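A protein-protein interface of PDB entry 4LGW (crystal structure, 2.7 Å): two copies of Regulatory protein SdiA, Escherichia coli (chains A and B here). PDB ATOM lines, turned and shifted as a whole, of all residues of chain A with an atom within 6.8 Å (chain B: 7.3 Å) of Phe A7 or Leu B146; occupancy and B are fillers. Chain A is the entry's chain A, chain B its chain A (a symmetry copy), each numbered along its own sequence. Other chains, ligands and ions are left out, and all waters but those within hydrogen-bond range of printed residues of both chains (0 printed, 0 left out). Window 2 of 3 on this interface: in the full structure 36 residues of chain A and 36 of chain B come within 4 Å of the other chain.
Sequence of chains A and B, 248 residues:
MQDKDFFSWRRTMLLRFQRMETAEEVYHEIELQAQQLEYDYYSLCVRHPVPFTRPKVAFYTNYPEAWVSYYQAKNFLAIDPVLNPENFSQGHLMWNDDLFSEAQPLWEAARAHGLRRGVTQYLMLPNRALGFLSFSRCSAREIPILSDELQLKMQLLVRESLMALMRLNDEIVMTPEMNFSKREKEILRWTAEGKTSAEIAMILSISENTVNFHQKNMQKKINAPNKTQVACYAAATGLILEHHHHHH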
ATOM      1  N   ASP A   5      19.874 -18.779   7.898  1.00  0.00           N
ATOM      2  CA  ASP A   5      19.652 -19.088   9.353  1.00  0.00           C
ATOM      3  C   ASP A   5      20.967 -19.144  10.171  1.00  0.00           C
ATOM      4  O   ASP A   5      21.907 -19.901   9.840  1.00  0.00           O
ATOM      5  CB  ASP A   5      18.835 -20.387   9.506  1.00  0.00           C
ATOM      6  CG  ASP A   5      18.564 -20.752  10.961  1.00  0.00           C
ATOM      7  OD1 ASP A   5      18.933 -21.884  11.330  1.00  0.00           O
ATOM      8  OD2 ASP A   5      17.993 -19.929  11.732  1.00  0.00           O
ATOM      9  N   PHE A   6      21.010 -18.350  11.248  1.00  0.00           N
ATOM     10  CA  PHE A   6      22.201 -18.254  12.106  1.00  0.00           C
ATOM     11  C   PHE A   6      22.688 -19.607  12.631  1.00  0.00           C
ATOM     12  O   PHE A   6      23.896 -19.865  12.652  1.00  0.00           O
ATOM     13  CB  PHE A   6      21.983 -17.266  13.270  1.00  0.00           C
ATOM     14  CG  PHE A   6      23.162 -17.176  14.238  1.00  0.00           C
ATOM     15  CD1 PHE A   6      24.431 -16.781  13.799  1.00  0.00           C
ATOM     16  CD2 PHE A   6      23.005 -17.486  15.594  1.00  0.00           C
ATOM     17  CE1 PHE A   6      25.527 -16.707  14.694  1.00  0.00           C
ATOM     18  CE2 PHE A   6      24.106 -17.416  16.488  1.00  0.00           C
ATOM     19  CZ  PHE A   6      25.359 -17.026  16.036  1.00  0.00           C
ATOM     20  N   PHE A   7      21.755 -20.468  13.044  1.00  0.00           N
ATOM     21  CA  PHE A   7      22.128 -21.724  13.713  1.00  0.00           C
ATOM     22  C   PHE A   7      23.042 -22.649  12.896  1.00  0.00           C
ATOM     23  O   PHE A   7      23.981 -23.236  13.452  1.00  0.00           O
ATOM     24  CB  PHE A   7      20.896 -22.498  14.206  1.00  0.00           C
ATOM     25  CG  PHE A   7      20.141 -21.835  15.340  1.00  0.00           C
ATOM     26  CD1 PHE A   7      20.776 -20.987  16.244  1.00  0.00           C
ATOM     27  CD2 PHE A   7      18.786 -22.110  15.534  1.00  0.00           C
ATOM     28  CE1 PHE A   7      20.072 -20.388  17.297  1.00  0.00           C
ATOM     29  CE2 PHE A   7      18.070 -21.518  16.591  1.00  0.00           C
ATOM     30  CZ  PHE A   7      18.721 -20.654  17.473  1.00  0.00           C
ATOM     31  N   SER A   8      22.770 -22.786  11.595  1.00  0.00           N
ATOM     32  CA  SER A   8      23.580 -23.682  10.752  1.00  0.00           C
ATOM     33  C   SER A   8      24.932 -23.063  10.387  1.00  0.00           C
ATOM     34  O   SER A   8      25.943 -23.784  10.212  1.00  0.00           O
ATOM     35  CB  SER A   8      22.825 -24.156   9.507  1.00  0.00           C
ATOM     36  OG  SER A   8      21.990 -23.127   9.031  1.00  0.00           O
ATOM     37  N   TRP A   9      24.944 -21.729  10.283  1.00  0.00           N
ATOM     38  CA  TRP A   9      26.194 -20.988  10.160  1.00  0.00           C
ATOM     39  C   TRP A   9      27.110 -21.389  11.315  1.00  0.00           C
ATOM     40  O   TRP A   9      28.191 -21.951  11.116  1.00  0.00           O
ATOM     41  CB  TRP A   9      25.935 -19.474  10.162  1.00  0.00           C
ATOM     42  CG  TRP A   9      27.184 -18.650   9.866  1.00  0.00           C
ATOM     43  CD1 TRP A   9      27.648 -18.276   8.639  1.00  0.00           C
ATOM     44  CD2 TRP A   9      28.121 -18.124  10.823  1.00  0.00           C
ATOM     45  NE1 TRP A   9      28.807 -17.548   8.770  1.00  0.00           N
ATOM     46  CE2 TRP A   9      29.121 -17.442  10.098  1.00  0.00           C
ATOM     47  CE3 TRP A   9      28.214 -18.168  12.221  1.00  0.00           C
ATOM     48  CZ2 TRP A   9      30.197 -16.815  10.719  1.00  0.00           C
ATOM     49  CZ3 TRP A   9      29.293 -17.535  12.840  1.00  0.00           C
ATOM     50  CH2 TRP A   9      30.263 -16.871  12.092  1.00  0.00           C
ATOM     51  N   ARG A  10      26.621 -21.118  12.522  1.00  0.00           N
ATOM     52  CA  ARG A  10      27.256 -21.486  13.769  1.00  0.00           C
ATOM     53  C   ARG A  10      27.796 -22.914  13.722  1.00  0.00           C
ATOM     54  O   ARG A  10      28.986 -23.146  13.937  1.00  0.00           O
ATOM     55  CB  ARG A  10      26.236 -21.315  14.890  1.00  0.00           C
ATOM     56  CG  ARG A  10      26.777 -21.474  16.278  1.00  0.00           C
ATOM     57  CD  ARG A  10      25.651 -21.584  17.298  1.00  0.00           C
ATOM     58  NE  ARG A  10      25.993 -22.541  18.349  1.00  0.00           N
ATOM     59  CZ  ARG A  10      26.782 -22.262  19.379  1.00  0.00           C
ATOM     60  NH1 ARG A  10      27.300 -21.039  19.506  1.00  0.00           N
ATOM     61  NH2 ARG A  10      27.053 -23.196  20.287  1.00  0.00           N
ATOM     62  N   ARG A  11      26.927 -23.865  13.406  1.00  0.00           N
ATOM     63  CA  ARG A  11      27.332 -25.261  13.374  1.00  0.00           C
ATOM     64  C   ARG A  11      28.405 -25.552  12.319  1.00  0.00           C
ATOM     65  O   ARG A  11      29.360 -26.301  12.600  1.00  0.00           O
ATOM     66  CB  ARG A  11      26.123 -26.186  13.241  1.00  0.00           C
ATOM     67  CG  ARG A  11      25.400 -26.424  14.583  1.00  0.00           C
ATOM     68  CD  ARG A  11      24.283 -27.496  14.506  1.00  0.00           C
ATOM     69  NE  ARG A  11      23.530 -27.384  13.250  1.00  0.00           N
ATOM     70  CZ  ARG A  11      22.476 -26.587  13.044  1.00  0.00           C
ATOM     71  NH1 ARG A  11      21.996 -25.822  14.025  1.00  0.00           N
ATOM     72  NH2 ARG A  11      21.892 -26.562  11.843  1.00  0.00           N
ATOM     73  N   THR A  12      28.267 -24.947  11.133  1.00  0.00           N
ATOM     74  CA  THR A  12      29.289 -25.073  10.093  1.00  0.00           C
ATOM     75  C   THR A  12      30.612 -24.531  10.618  1.00  0.00           C
ATOM     76  O   THR A  12      31.654 -25.214  10.558  1.00  0.00           O
ATOM     77  CB  THR A  12      28.894 -24.347   8.778  1.00  0.00           C
ATOM     78  OG1 THR A  12      27.860 -25.074   8.112  1.00  0.00           O
ATOM     79  CG2 THR A  12      30.081 -24.243   7.822  1.00  0.00           C
ATOM     80  N   PHE B   6      15.163 -15.603  17.806  1.00  0.00           N
ATOM     81  CA  PHE B   6      16.198 -15.491  18.846  1.00  0.00           C
ATOM     82  C   PHE B   6      16.642 -14.050  19.114  1.00  0.00           C
ATOM     83  O   PHE B   6      16.820 -13.663  20.274  1.00  0.00           O
ATOM     84  CB  PHE B   6      17.414 -16.385  18.532  1.00  0.00           C
ATOM     85  CG  PHE B   6      18.556 -16.258  19.543  1.00  0.00           C
ATOM     86  CD1 PHE B   6      18.361 -16.552  20.897  1.00  0.00           C
ATOM     87  CD2 PHE B   6      19.830 -15.843  19.139  1.00  0.00           C
ATOM     88  CE1 PHE B   6      19.414 -16.426  21.834  1.00  0.00           C
ATOM     89  CE2 PHE B   6      20.884 -15.712  20.081  1.00  0.00           C
ATOM     90  CZ  PHE B   6      20.673 -16.005  21.422  1.00  0.00           C
ATOM     91  N   ILE B 143      11.157 -33.563  26.731  1.00  0.00           N
ATOM     92  CA  ILE B 143      10.747 -32.239  26.224  1.00  0.00           C
ATOM     93  C   ILE B 143      11.632 -31.793  25.042  1.00  0.00           C
ATOM     94  O   ILE B 143      12.703 -31.217  25.260  1.00  0.00           O
ATOM     95  CB  ILE B 143      10.634 -31.171  27.361  1.00  0.00           C
ATOM     96  CG1 ILE B 143       9.480 -31.548  28.306  1.00  0.00           C
ATOM     97  CG2 ILE B 143      10.422 -29.748  26.781  1.00  0.00           C
ATOM     98  CD1 ILE B 143       9.668 -31.142  29.765  1.00  0.00           C
ATOM     99  N   PRO B 144      11.188 -32.069  23.785  1.00  0.00           N
ATOM    100  CA  PRO B 144      12.002 -31.691  22.608  1.00  0.00           C
ATOM    101  C   PRO B 144      12.308 -30.178  22.567  1.00  0.00           C
ATOM    102  O   PRO B 144      11.393 -29.361  22.415  1.00  0.00           O
ATOM    103  CB  PRO B 144      11.123 -32.109  21.406  1.00  0.00           C
ATOM    104  CG  PRO B 144       9.726 -32.229  21.965  1.00  0.00           C
ATOM    105  CD  PRO B 144       9.920 -32.717  23.382  1.00  0.00           C
ATOM    106  N   ILE B 145      13.573 -29.810  22.762  1.00  0.00           N
ATOM    107  CA  ILE B 145      14.011 -28.429  22.535  1.00  0.00           C
ATOM    108  C   ILE B 145      15.224 -28.486  21.639  1.00  0.00           C
ATOM    109  O   ILE B 145      16.052 -29.395  21.776  1.00  0.00           O
ATOM    110  CB  ILE B 145      14.333 -27.643  23.851  1.00  0.00           C
ATOM    111  CG1 ILE B 145      14.249 -26.123  23.619  1.00  0.00           C
ATOM    112  CG2 ILE B 145      15.688 -28.038  24.432  1.00  0.00           C
ATOM    113  CD1 ILE B 145      12.805 -25.572  23.554  1.00  0.00           C
ATOM    114  N   LEU B 146      15.322 -27.539  20.708  1.00  0.00           N
ATOM    115  CA  LEU B 146      16.477 -27.522  19.819  1.00  0.00           C
ATOM    116  C   LEU B 146      17.731 -27.275  20.655  1.00  0.00           C
ATOM    117  O   LEU B 146      17.822 -26.288  21.399  1.00  0.00           O
ATOM    118  CB  LEU B 146      16.328 -26.504  18.679  1.00  0.00           C
ATOM    119  CG  LEU B 146      17.326 -26.698  17.523  1.00  0.00           C
ATOM    120  CD1 LEU B 146      17.247 -28.119  16.899  1.00  0.00           C
ATOM    121  CD2 LEU B 146      17.156 -25.607  16.457  1.00  0.00           C
ATOM    122  N   SER B 147      18.672 -28.207  20.560  1.00  0.00           N
ATOM    123  CA  SER B 147      19.915 -28.113  21.302  1.00  0.00           C
ATOM    124  C   SER B 147      20.505 -26.702  21.227  1.00  0.00           C
ATOM    125  O   SER B 147      20.860 -26.107  22.247  1.00  0.00           O
ATOM    126  CB  SER B 147      20.910 -29.123  20.745  1.00  0.00           C
ATOM    127  OG  SER B 147      22.141 -29.013  21.418  1.00  0.00           O
ATOM    128  N   ASP B 148      20.569 -26.171  20.007  1.00  0.00           N
ATOM    129  CA  ASP B 148      21.223 -24.903  19.720  1.00  0.00           C
ATOM    130  C   ASP B 148      20.547 -23.714  20.399  1.00  0.00           C
ATOM    131  O   ASP B 148      21.218 -22.770  20.814  1.00  0.00           O
ATOM    132  CB  ASP B 148      21.323 -24.685  18.203  1.00  0.00           C
ATOM    133  CG  ASP B 148      21.967 -25.868  17.471  1.00  0.00           C
ATOM    134  OD1 ASP B 148      21.444 -26.244  16.408  1.00  0.00           O
ATOM    135  OD2 ASP B 148      22.981 -26.435  17.944  1.00  0.00           O
ATOM    136  N   GLU B 149      19.225 -23.772  20.511  1.00  0.00           N
ATOM    137  CA  GLU B 149      18.447 -22.712  21.139  1.00  0.00           C
ATOM    138  C   GLU B 149      18.697 -22.660  22.650  1.00  0.00           C
ATOM    139  O   GLU B 149      18.886 -21.585  23.223  1.00  0.00           O
ATOM    140  CB  GLU B 149      16.954 -22.908  20.857  1.00  0.00           C
ATOM    141  CG  GLU B 149      16.080 -21.737  21.295  1.00  0.00           C
ATOM    142  CD  GLU B 149      14.606 -22.106  21.493  1.00  0.00           C
ATOM    143  OE1 GLU B 149      14.007 -21.677  22.514  1.00  0.00           O
ATOM    144  OE2 GLU B 149      14.045 -22.813  20.623  1.00  0.00           O
ATOM    145  N   LEU B 150      18.694 -23.824  23.293  1.00  0.00           N
ATOM    146  CA  LEU B 150      18.856 -23.898  24.736  1.00  0.00           C
ATOM    147  C   LEU B 150      20.211 -23.298  25.083  1.00  0.00           C
ATOM    148  O   LEU B 150      20.330 -22.377  25.911  1.00  0.00           O
ATOM    149  CB  LEU B 150      18.772 -25.354  25.204  1.00  0.00           C
ATOM    150  CG  LEU B 150      18.884 -25.608  26.710  1.00  0.00           C
ATOM    151  CD1 LEU B 150      17.705 -24.997  27.455  1.00  0.00           C
ATOM    152  CD2 LEU B 150      19.018 -27.094  26.994  1.00  0.00           C
ATOM    153  N   GLN B 151      21.213 -23.821  24.396  1.00  0.00           N
ATOM    154  CA  GLN B 151      22.581 -23.404  24.529  1.00  0.00           C
ATOM    155  C   GLN B 151      22.743 -21.889  24.480  1.00  0.00           C
ATOM    156  O   GLN B 151      23.259 -21.266  25.419  1.00  0.00           O
ATOM    157  CB  GLN B 151      23.334 -24.003  23.376  1.00  0.00           C
ATOM    158  CG  GLN B 151      24.657 -24.502  23.772  1.00  0.00           C
ATOM    159  CD  GLN B 151      25.182 -25.472  22.775  1.00  0.00           C
ATOM    160  OE1 GLN B 151      24.445 -26.318  22.266  1.00  0.00           O
ATOM    161  NE2 GLN B 151      26.464 -25.357  22.475  1.00  0.00           N
ATOM    162  N   LEU B 152      22.305 -21.298  23.374  1.00  0.00           N
ATOM    163  CA  LEU B 152      22.444 -19.873  23.216  1.00  0.00           C
ATOM    164  C   LEU B 152      21.668 -19.091  24.248  1.00  0.00           C
ATOM    165  O   LEU B 152      22.143 -18.058  24.712  1.00  0.00           O
ATOM    166  CB  LEU B 152      22.072 -19.427  21.817  1.00  0.00           C
ATOM    167  CG  LEU B 152      23.274 -19.148  20.915  1.00  0.00           C
ATOM    168  CD1 LEU B 152      23.930 -20.422  20.391  1.00  0.00           C
ATOM    169  CD2 LEU B 152      22.771 -18.327  19.766  1.00  0.00           C
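NH2 of Arg A10 lies close to NE2 of Gln B151 (3.1 Å). NH1 of Arg A11 lies within salt-bridge range of OD1 of Asp B148 (2.5 Å).
Hydrophobic or aromatic side chains of chain B that line the printed part of chain A: Leu B146 and Leu B152. Hydrophobic or aromatic side chains of chain A that line the printed part of chain B: Phe A6 and Phe A7.
Phe A7 touches just one residue of chain B: Leu B146 (3.97 Å). Leu B146 touches just one residue of chain A: Phe A7. Printed residues of chain B within 4 Å of Arg A11: Asp B148 (2.5 Å). Of the printed residues of chain B, Arg A10 touches Gln B151 and Leu B152. Of the printed residues of chain A, Leu B152 touches Phe A6 (3.7 Å) and Arg A10 (3.5 Å). Of the printed residues of chain A, Asp B148 touches Arg A11. Of the printed residues of chain B, Phe A6 touches Leu B152. Thr A12 touches none of the printed residues of chain B. Asp A5 touches none of the printed residues of chain B. The nearest printed residue of chain B that does not touch Phe A7 is Leu B152 (4.2 Å). The nearest residue of chain A that does not touch Leu B146 is Arg A11 (5.4 Å).
Position printed for both chains: 6.
CD2 of Leu B152 touches CE2 of Phe A6, 3.7 Å away. Phe A7 touches Leu B146 (CD2 to CD2, 3.97 Å). NH1 of Arg A10 touches CD1 of Leu B152 (3.5 Å).
O of Phe A7 is in hydrogen-bond range of NH1 of Arg A11 (3.3 Å).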
